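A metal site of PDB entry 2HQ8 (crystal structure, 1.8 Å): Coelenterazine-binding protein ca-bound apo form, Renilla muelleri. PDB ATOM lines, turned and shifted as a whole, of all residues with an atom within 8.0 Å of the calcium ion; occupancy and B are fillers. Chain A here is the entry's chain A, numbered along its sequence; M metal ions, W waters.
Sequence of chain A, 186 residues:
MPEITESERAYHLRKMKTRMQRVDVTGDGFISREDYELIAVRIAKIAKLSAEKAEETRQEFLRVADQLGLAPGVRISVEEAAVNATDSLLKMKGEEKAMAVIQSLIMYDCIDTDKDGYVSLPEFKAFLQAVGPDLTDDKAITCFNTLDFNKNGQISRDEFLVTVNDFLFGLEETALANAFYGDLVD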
ATOM      1  N   MET A  20     -27.349  23.376 -22.919  1.00  0.00           N
ATOM      2  CA  MET A  20     -27.250  22.795 -21.561  1.00  0.00           C
ATOM      3  C   MET A  20     -25.830  22.896 -20.969  1.00  0.00           C
ATOM      4  O   MET A  20     -25.639  23.237 -19.799  1.00  0.00           O
ATOM      5  CB  MET A  20     -27.780  21.340 -21.558  1.00  0.00           C
ATOM      6  CG  MET A  20     -29.209  21.182 -22.072  1.00  0.00           C
ATOM      7  SD  MET A  20     -30.383  22.385 -21.463  1.00  0.00           S
ATOM      8  CE  MET A  20     -31.781  21.994 -22.480  1.00  0.00           C
ATOM      9  N   GLN A  21     -24.810  22.677 -21.790  1.00  0.00           N
ATOM     10  CA  GLN A  21     -23.434  22.828 -21.299  1.00  0.00           C
ATOM     11  C   GLN A  21     -23.094  24.254 -20.900  1.00  0.00           C
ATOM     12  O   GLN A  21     -22.486  24.476 -19.880  1.00  0.00           O
ATOM     13  CB  GLN A  21     -22.428  22.277 -22.300  1.00  0.00           C
ATOM     14  CG  GLN A  21     -22.490  20.752 -22.354  1.00  0.00           C
ATOM     15  CD  GLN A  21     -21.443  20.156 -23.263  1.00  0.00           C
ATOM     16  OE1 GLN A  21     -20.413  20.771 -23.524  1.00  0.00           O
ATOM     17  NE2 GLN A  21     -21.709  18.954 -23.776  1.00  0.00           N
ATOM     18  N   VAL A  23     -25.354  26.518 -19.851  1.00  0.00           N
ATOM     19  CA  VAL A  23     -26.178  26.798 -18.660  1.00  0.00           C
ATOM     20  C   VAL A  23     -25.535  26.156 -17.435  1.00  0.00           C
ATOM     21  O   VAL A  23     -25.539  26.731 -16.354  1.00  0.00           O
ATOM     22  CB  VAL A  23     -27.671  26.392 -18.818  1.00  0.00           C
ATOM     23  CG1 VAL A  23     -28.457  26.539 -17.486  1.00  0.00           C
ATOM     24  CG2 VAL A  23     -28.345  27.259 -19.940  1.00  0.00           C
ATOM     25  N   ASP A  24     -24.920  24.994 -17.626  1.00  0.00           N
ATOM     26  CA  ASP A  24     -24.193  24.351 -16.497  1.00  0.00           C
ATOM     27  C   ASP A  24     -22.884  25.081 -16.151  1.00  0.00           C
ATOM     28  O   ASP A  24     -21.776  24.555 -16.400  1.00  0.00           O
ATOM     29  CB  ASP A  24     -23.912  22.877 -16.765  1.00  0.00           C
ATOM     30  CG  ASP A  24     -23.150  22.205 -15.614  1.00  0.00           C
ATOM     31  OD1 ASP A  24     -23.150  22.737 -14.486  1.00  0.00           O
ATOM     32  OD2 ASP A  24     -22.545  21.151 -15.851  1.00  0.00           O
ATOM     33  N   VAL A  25     -23.020  26.250 -15.548  1.00  0.00           N
ATOM     34  CA  VAL A  25     -21.858  27.039 -15.117  1.00  0.00           C
ATOM     35  C   VAL A  25     -21.188  26.454 -13.893  1.00  0.00           C
ATOM     36  O   VAL A  25     -19.989  26.692 -13.690  1.00  0.00           O
ATOM     37  CB  VAL A  25     -22.173  28.521 -14.916  1.00  0.00           C
ATOM     38  CG1 VAL A  25     -22.376  29.182 -16.307  1.00  0.00           C
ATOM     39  CG2 VAL A  25     -23.414  28.729 -13.990  1.00  0.00           C
ATOM     40  N   THR A  26     -21.936  25.695 -13.080  1.00  0.00           N
ATOM     41  CA  THR A  26     -21.292  25.072 -11.915  1.00  0.00           C
ATOM     42  C   THR A  26     -20.371  23.906 -12.268  1.00  0.00           C
ATOM     43  O   THR A  26     -19.554  23.500 -11.437  1.00  0.00           O
ATOM     44  CB  THR A  26     -22.260  24.637 -10.798  1.00  0.00           C
ATOM     45  OG1 THR A  26     -23.037  23.513 -11.225  1.00  0.00           O
ATOM     46  CG2 THR A  26     -23.109  25.789 -10.322  1.00  0.00           C
ATOM     47  N   GLY A  27     -20.512  23.358 -13.479  1.00  0.00           N
ATOM     48  CA  GLY A  27     -19.637  22.311 -14.025  1.00  0.00           C
ATOM     49  C   GLY A  27     -19.757  20.909 -13.415  1.00  0.00           C
ATOM     50  O   GLY A  27     -18.836  20.086 -13.555  1.00  0.00           O
ATOM     51  N   ASP A  28     -20.891  20.646 -12.754  1.00  0.00           N
ATOM     52  CA  ASP A  28     -21.227  19.332 -12.163  1.00  0.00           C
ATOM     53  C   ASP A  28     -21.942  18.361 -13.112  1.00  0.00           C
ATOM     54  O   ASP A  28     -22.212  17.200 -12.741  1.00  0.00           O
ATOM     55  CB  ASP A  28     -22.029  19.545 -10.850  1.00  0.00           C
ATOM     56  CG  ASP A  28     -23.426  20.116 -11.099  1.00  0.00           C
ATOM     57  OD1 ASP A  28     -23.670  20.700 -12.203  1.00  0.00           O
ATOM     58  OD2 ASP A  28     -24.311  19.964 -10.220  1.00  0.00           O
ATOM     59  N   GLY A  29     -22.237  18.808 -14.342  1.00  0.00           N
ATOM     60  CA  GLY A  29     -22.891  17.978 -15.352  1.00  0.00           C
ATOM     61  C   GLY A  29     -24.415  17.915 -15.194  1.00  0.00           C
ATOM     62  O   GLY A  29     -25.090  17.085 -15.813  1.00  0.00           O
ATOM     63  N   PHE A  30     -24.920  18.825 -14.375  1.00  0.00           N
ATOM     64  CA  PHE A  30     -26.354  19.016 -14.146  1.00  0.00           C
ATOM     65  C   PHE A  30     -26.753  20.493 -14.297  1.00  0.00           C
ATOM     66  O   PHE A  30     -25.936  21.407 -14.153  1.00  0.00           O
ATOM     67  CB  PHE A  30     -26.701  18.611 -12.718  1.00  0.00           C
ATOM     68  CG  PHE A  30     -26.568  17.145 -12.472  1.00  0.00           C
ATOM     69  CD1 PHE A  30     -27.644  16.287 -12.755  1.00  0.00           C
ATOM     70  CD2 PHE A  30     -25.376  16.608 -12.017  1.00  0.00           C
ATOM     71  CE1 PHE A  30     -27.534  14.901 -12.554  1.00  0.00           C
ATOM     72  CE2 PHE A  30     -25.245  15.222 -11.823  1.00  0.00           C
ATOM     73  CZ  PHE A  30     -26.329  14.369 -12.101  1.00  0.00           C
ATOM     74  N   ILE A  31     -28.047  20.677 -14.532  1.00  0.00           N
ATOM     75  CA  ILE A  31     -28.700  21.979 -14.537  1.00  0.00           C
ATOM     76  C   ILE A  31     -29.548  22.058 -13.256  1.00  0.00           C
ATOM     77  O   ILE A  31     -30.369  21.185 -13.016  1.00  0.00           O
ATOM     78  CB  ILE A  31     -29.642  22.132 -15.753  1.00  0.00           C
ATOM     79  CG1 ILE A  31     -28.884  22.031 -17.088  1.00  0.00           C
ATOM     80  CG2 ILE A  31     -30.454  23.467 -15.647  1.00  0.00           C
ATOM     81  CD1 ILE A  31     -27.633  22.868 -17.147  1.00  0.00           C
ATOM     82  N   SER A  32     -29.343  23.132 -12.489  1.00  0.00           N
ATOM     83  CA  SER A  32     -30.020  23.403 -11.229  1.00  0.00           C
ATOM     84  C   SER A  32     -30.148  24.915 -11.010  1.00  0.00           C
ATOM     85  O   SER A  32     -29.542  25.758 -11.750  1.00  0.00           O
ATOM     86  CB  SER A  32     -29.280  22.706 -10.073  1.00  0.00           C
ATOM     87  OG  SER A  32     -28.044  23.344  -9.754  1.00  0.00           O
ATOM     88  N   ARG A  33     -30.915  25.299  -9.991  1.00  0.00           N
ATOM     89  CA  ARG A  33     -31.044  26.736  -9.729  1.00  0.00           C
ATOM     90  C   ARG A  33     -29.706  27.396  -9.381  1.00  0.00           C
ATOM     91  O   ARG A  33     -29.531  28.574  -9.645  1.00  0.00           O
ATOM     92  CB  ARG A  33     -32.075  26.989  -8.643  1.00  0.00           C
ATOM     93  CG  ARG A  33     -31.673  26.523  -7.267  1.00  0.00           C
ATOM     94  CD  ARG A  33     -32.901  26.579  -6.319  1.00  0.00           C
ATOM     95  NE  ARG A  33     -33.355  27.947  -6.021  1.00  0.00           N
ATOM     96  CZ  ARG A  33     -34.449  28.542  -6.509  1.00  0.00           C
ATOM     97  NH1 ARG A  33     -35.226  27.952  -7.392  1.00  0.00           N
ATOM     98  NH2 ARG A  33     -34.756  29.765  -6.108  1.00  0.00           N
ATOM     99  N   GLU A  34     -28.777  26.631  -8.793  1.00  0.00           N
ATOM    100  CA  GLU A  34     -27.408  27.091  -8.547  1.00  0.00           C
ATOM    101  C   GLU A  34     -26.739  27.669  -9.793  1.00  0.00           C
ATOM    102  O   GLU A  34     -26.007  28.676  -9.682  1.00  0.00           O
ATOM    103  CB  GLU A  34     -26.549  25.949  -7.996  1.00  0.00           C
ATOM    104  CG  GLU A  34     -26.923  25.534  -6.518  1.00  0.00           C
ATOM    105  CD  GLU A  34     -28.137  24.583  -6.378  1.00  0.00           C
ATOM    106  OE1 GLU A  34     -28.690  24.073  -7.355  1.00  0.00           O
ATOM    107  OE2 GLU A  34     -28.540  24.365  -5.220  1.00  0.00           O
ATOM    108  N   ASP A  35     -26.962  27.022 -10.951  1.00  0.00           N
ATOM    109  CA  ASP A  35     -26.490  27.531 -12.268  1.00  0.00           C
ATOM    110  C   ASP A  35     -27.058  28.919 -12.602  1.00  0.00           C
ATOM    111  O   ASP A  35     -26.317  29.835 -12.959  1.00  0.00           O
ATOM    112  CB  ASP A  35     -26.807  26.540 -13.402  1.00  0.00           C
ATOM    113  CG  ASP A  35     -26.095  25.218 -13.228  1.00  0.00           C
ATOM    114  OD1 ASP A  35     -24.848  25.239 -13.104  1.00  0.00           O
ATOM    115  OD2 ASP A  35     -26.760  24.149 -13.206  1.00  0.00           O
ATOM    116  N   TYR A  36     -28.383  29.035 -12.561  1.00  0.00           N
ATOM    117  CA  TYR A  36     -29.026  30.332 -12.769  1.00  0.00           C
ATOM    118  C   TYR A  36     -28.508  31.387 -11.823  1.00  0.00           C
ATOM    119  O   TYR A  36     -28.216  32.502 -12.249  1.00  0.00           O
ATOM    120  CB  TYR A  36     -30.570  30.217 -12.714  1.00  0.00           C
ATOM    121  CG  TYR A  36     -31.061  29.572 -13.978  1.00  0.00           C
ATOM    122  CD1 TYR A  36     -30.930  28.195 -14.198  1.00  0.00           C
ATOM    123  CD2 TYR A  36     -31.634  30.340 -15.007  1.00  0.00           C
ATOM    124  CE1 TYR A  36     -31.334  27.606 -15.354  1.00  0.00           C
ATOM    125  CE2 TYR A  36     -32.072  29.731 -16.185  1.00  0.00           C
ATOM    126  CZ  TYR A  36     -31.904  28.360 -16.343  1.00  0.00           C
ATOM    127  OH  TYR A  36     -32.292  27.746 -17.493  1.00  0.00           O
ATOM    128  N   LEU A  38     -25.558  31.481 -10.297  1.00  0.00           N
ATOM    129  CA  LEU A  38     -24.174  31.798 -10.643  1.00  0.00           C
ATOM    130  C   LEU A  38     -24.041  32.667 -11.906  1.00  0.00           C
ATOM    131  O   LEU A  38     -23.164  33.533 -11.969  1.00  0.00           O
ATOM    132  CB  LEU A  38     -23.346  30.535 -10.809  1.00  0.00           C
ATOM    133  CG  LEU A  38     -21.842  30.716 -11.062  1.00  0.00           C
ATOM    134  CD1 LEU A  38     -21.210  31.673 -10.049  1.00  0.00           C
ATOM    135  CD2 LEU A  38     -21.180  29.332 -11.126  1.00  0.00           C
ATOM    136  N   ARG A  75     -32.142  18.684  -9.746  1.00  0.00           N
ATOM    137  CA  ARG A  75     -30.972  18.692 -10.655  1.00  0.00           C
ATOM    138  C   ARG A  75     -31.315  17.792 -11.827  1.00  0.00           C
ATOM    139  O   ARG A  75     -31.642  16.597 -11.620  1.00  0.00           O
ATOM    140  CB  ARG A  75     -29.712  18.108  -9.965  1.00  0.00           C
ATOM    141  CG  ARG A  75     -29.130  18.883  -8.789  1.00  0.00           C
ATOM    142  CD  ARG A  75     -27.818  18.188  -8.289  1.00  0.00           C
ATOM    143  NE  ARG A  75     -28.120  16.831  -7.824  1.00  0.00           N
ATOM    144  CZ  ARG A  75     -27.329  15.764  -7.982  1.00  0.00           C
ATOM    145  NH1 ARG A  75     -26.148  15.862  -8.615  1.00  0.00           N
ATOM    146  NH2 ARG A  75     -27.731  14.587  -7.522  1.00  0.00           N
ATOM    147  N   ILE A  76     -31.198  18.309 -13.049  1.00  0.00           N
ATOM    148  CA  ILE A  76     -31.384  17.491 -14.259  1.00  0.00           C
ATOM    149  C   ILE A  76     -30.049  17.397 -15.002  1.00  0.00           C
ATOM    150  O   ILE A  76     -29.415  18.440 -15.262  1.00  0.00           O
ATOM    151  CB  ILE A  76     -32.431  18.109 -15.226  1.00  0.00           C
ATOM    152  CG1 ILE A  76     -33.748  18.441 -14.481  1.00  0.00           C
ATOM    153  CG2 ILE A  76     -32.637  17.231 -16.439  1.00  0.00           C
ATOM    154  CD1 ILE A  76     -34.424  17.274 -13.714  1.00  0.00           C
ATOM    155  N   VAL A  78     -27.224  17.250 -17.828  1.00  0.00           N
ATOM    156  CA  VAL A  78     -27.130  17.966 -19.114  1.00  0.00           C
ATOM    157  C   VAL A  78     -27.486  17.063 -20.284  1.00  0.00           C
ATOM    158  O   VAL A  78     -28.100  17.486 -21.282  1.00  0.00           O
ATOM    159  CB  VAL A  78     -25.739  18.677 -19.303  1.00  0.00           C
ATOM    160  CG1 VAL A  78     -25.585  19.798 -18.309  1.00  0.00           C
ATOM    161  CG2 VAL A  78     -24.579  17.690 -19.201  1.00  0.00           C
HETATM  162 CA    CA M   1     -24.758  22.797 -12.761  1.00  0.00          CA
HETATM  163  O   HOH W   1     -26.020  22.050 -10.881  1.00  0.00           O
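The side-chain carboxylate (OD1) of Asp 24 sits close to the backbone NH (N) of Gly 27 (2.9 Å).
The backbone NH (N) of Gly 29 sits at hydrogen-bond distance from the side-chain carboxylate (OD2) of Asp 24, at 2.8 Å.
The side-chain carboxylate (OD2) of Asp 35 sits close to the backbone NH (N) of Ser 32, 2.9 Å away.
The side-chain carboxylate (OD1) of Asp 35 sits close to the backbone NH (N) of Val 25 (3.2 Å).
Water W1 lies within hydrogen-bond range of OG of Ser 32 and OD2 of Asp 28.
Five residues have an atom within 4 Å of the calcium ion: Asp 24, Thr 26, Asp 28, Phe 30 and Asp 35.
Along chain A the residues within 4 Å of the calcium ion span positions 24 to 35.
The calcium ion is bound by the backbone carbonyl oxygen (O) of Phe 30, the side-chain carboxylate (OD1) of Asp 24, water W1, the side-chain hydroxyl (OG1) of Thr 26, the side-chain carboxylate (OD1) of Asp 28, the side-chain carboxylate (OD2) of Asp 35 and the side-chain carboxylate (OD1) of Asp 35.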
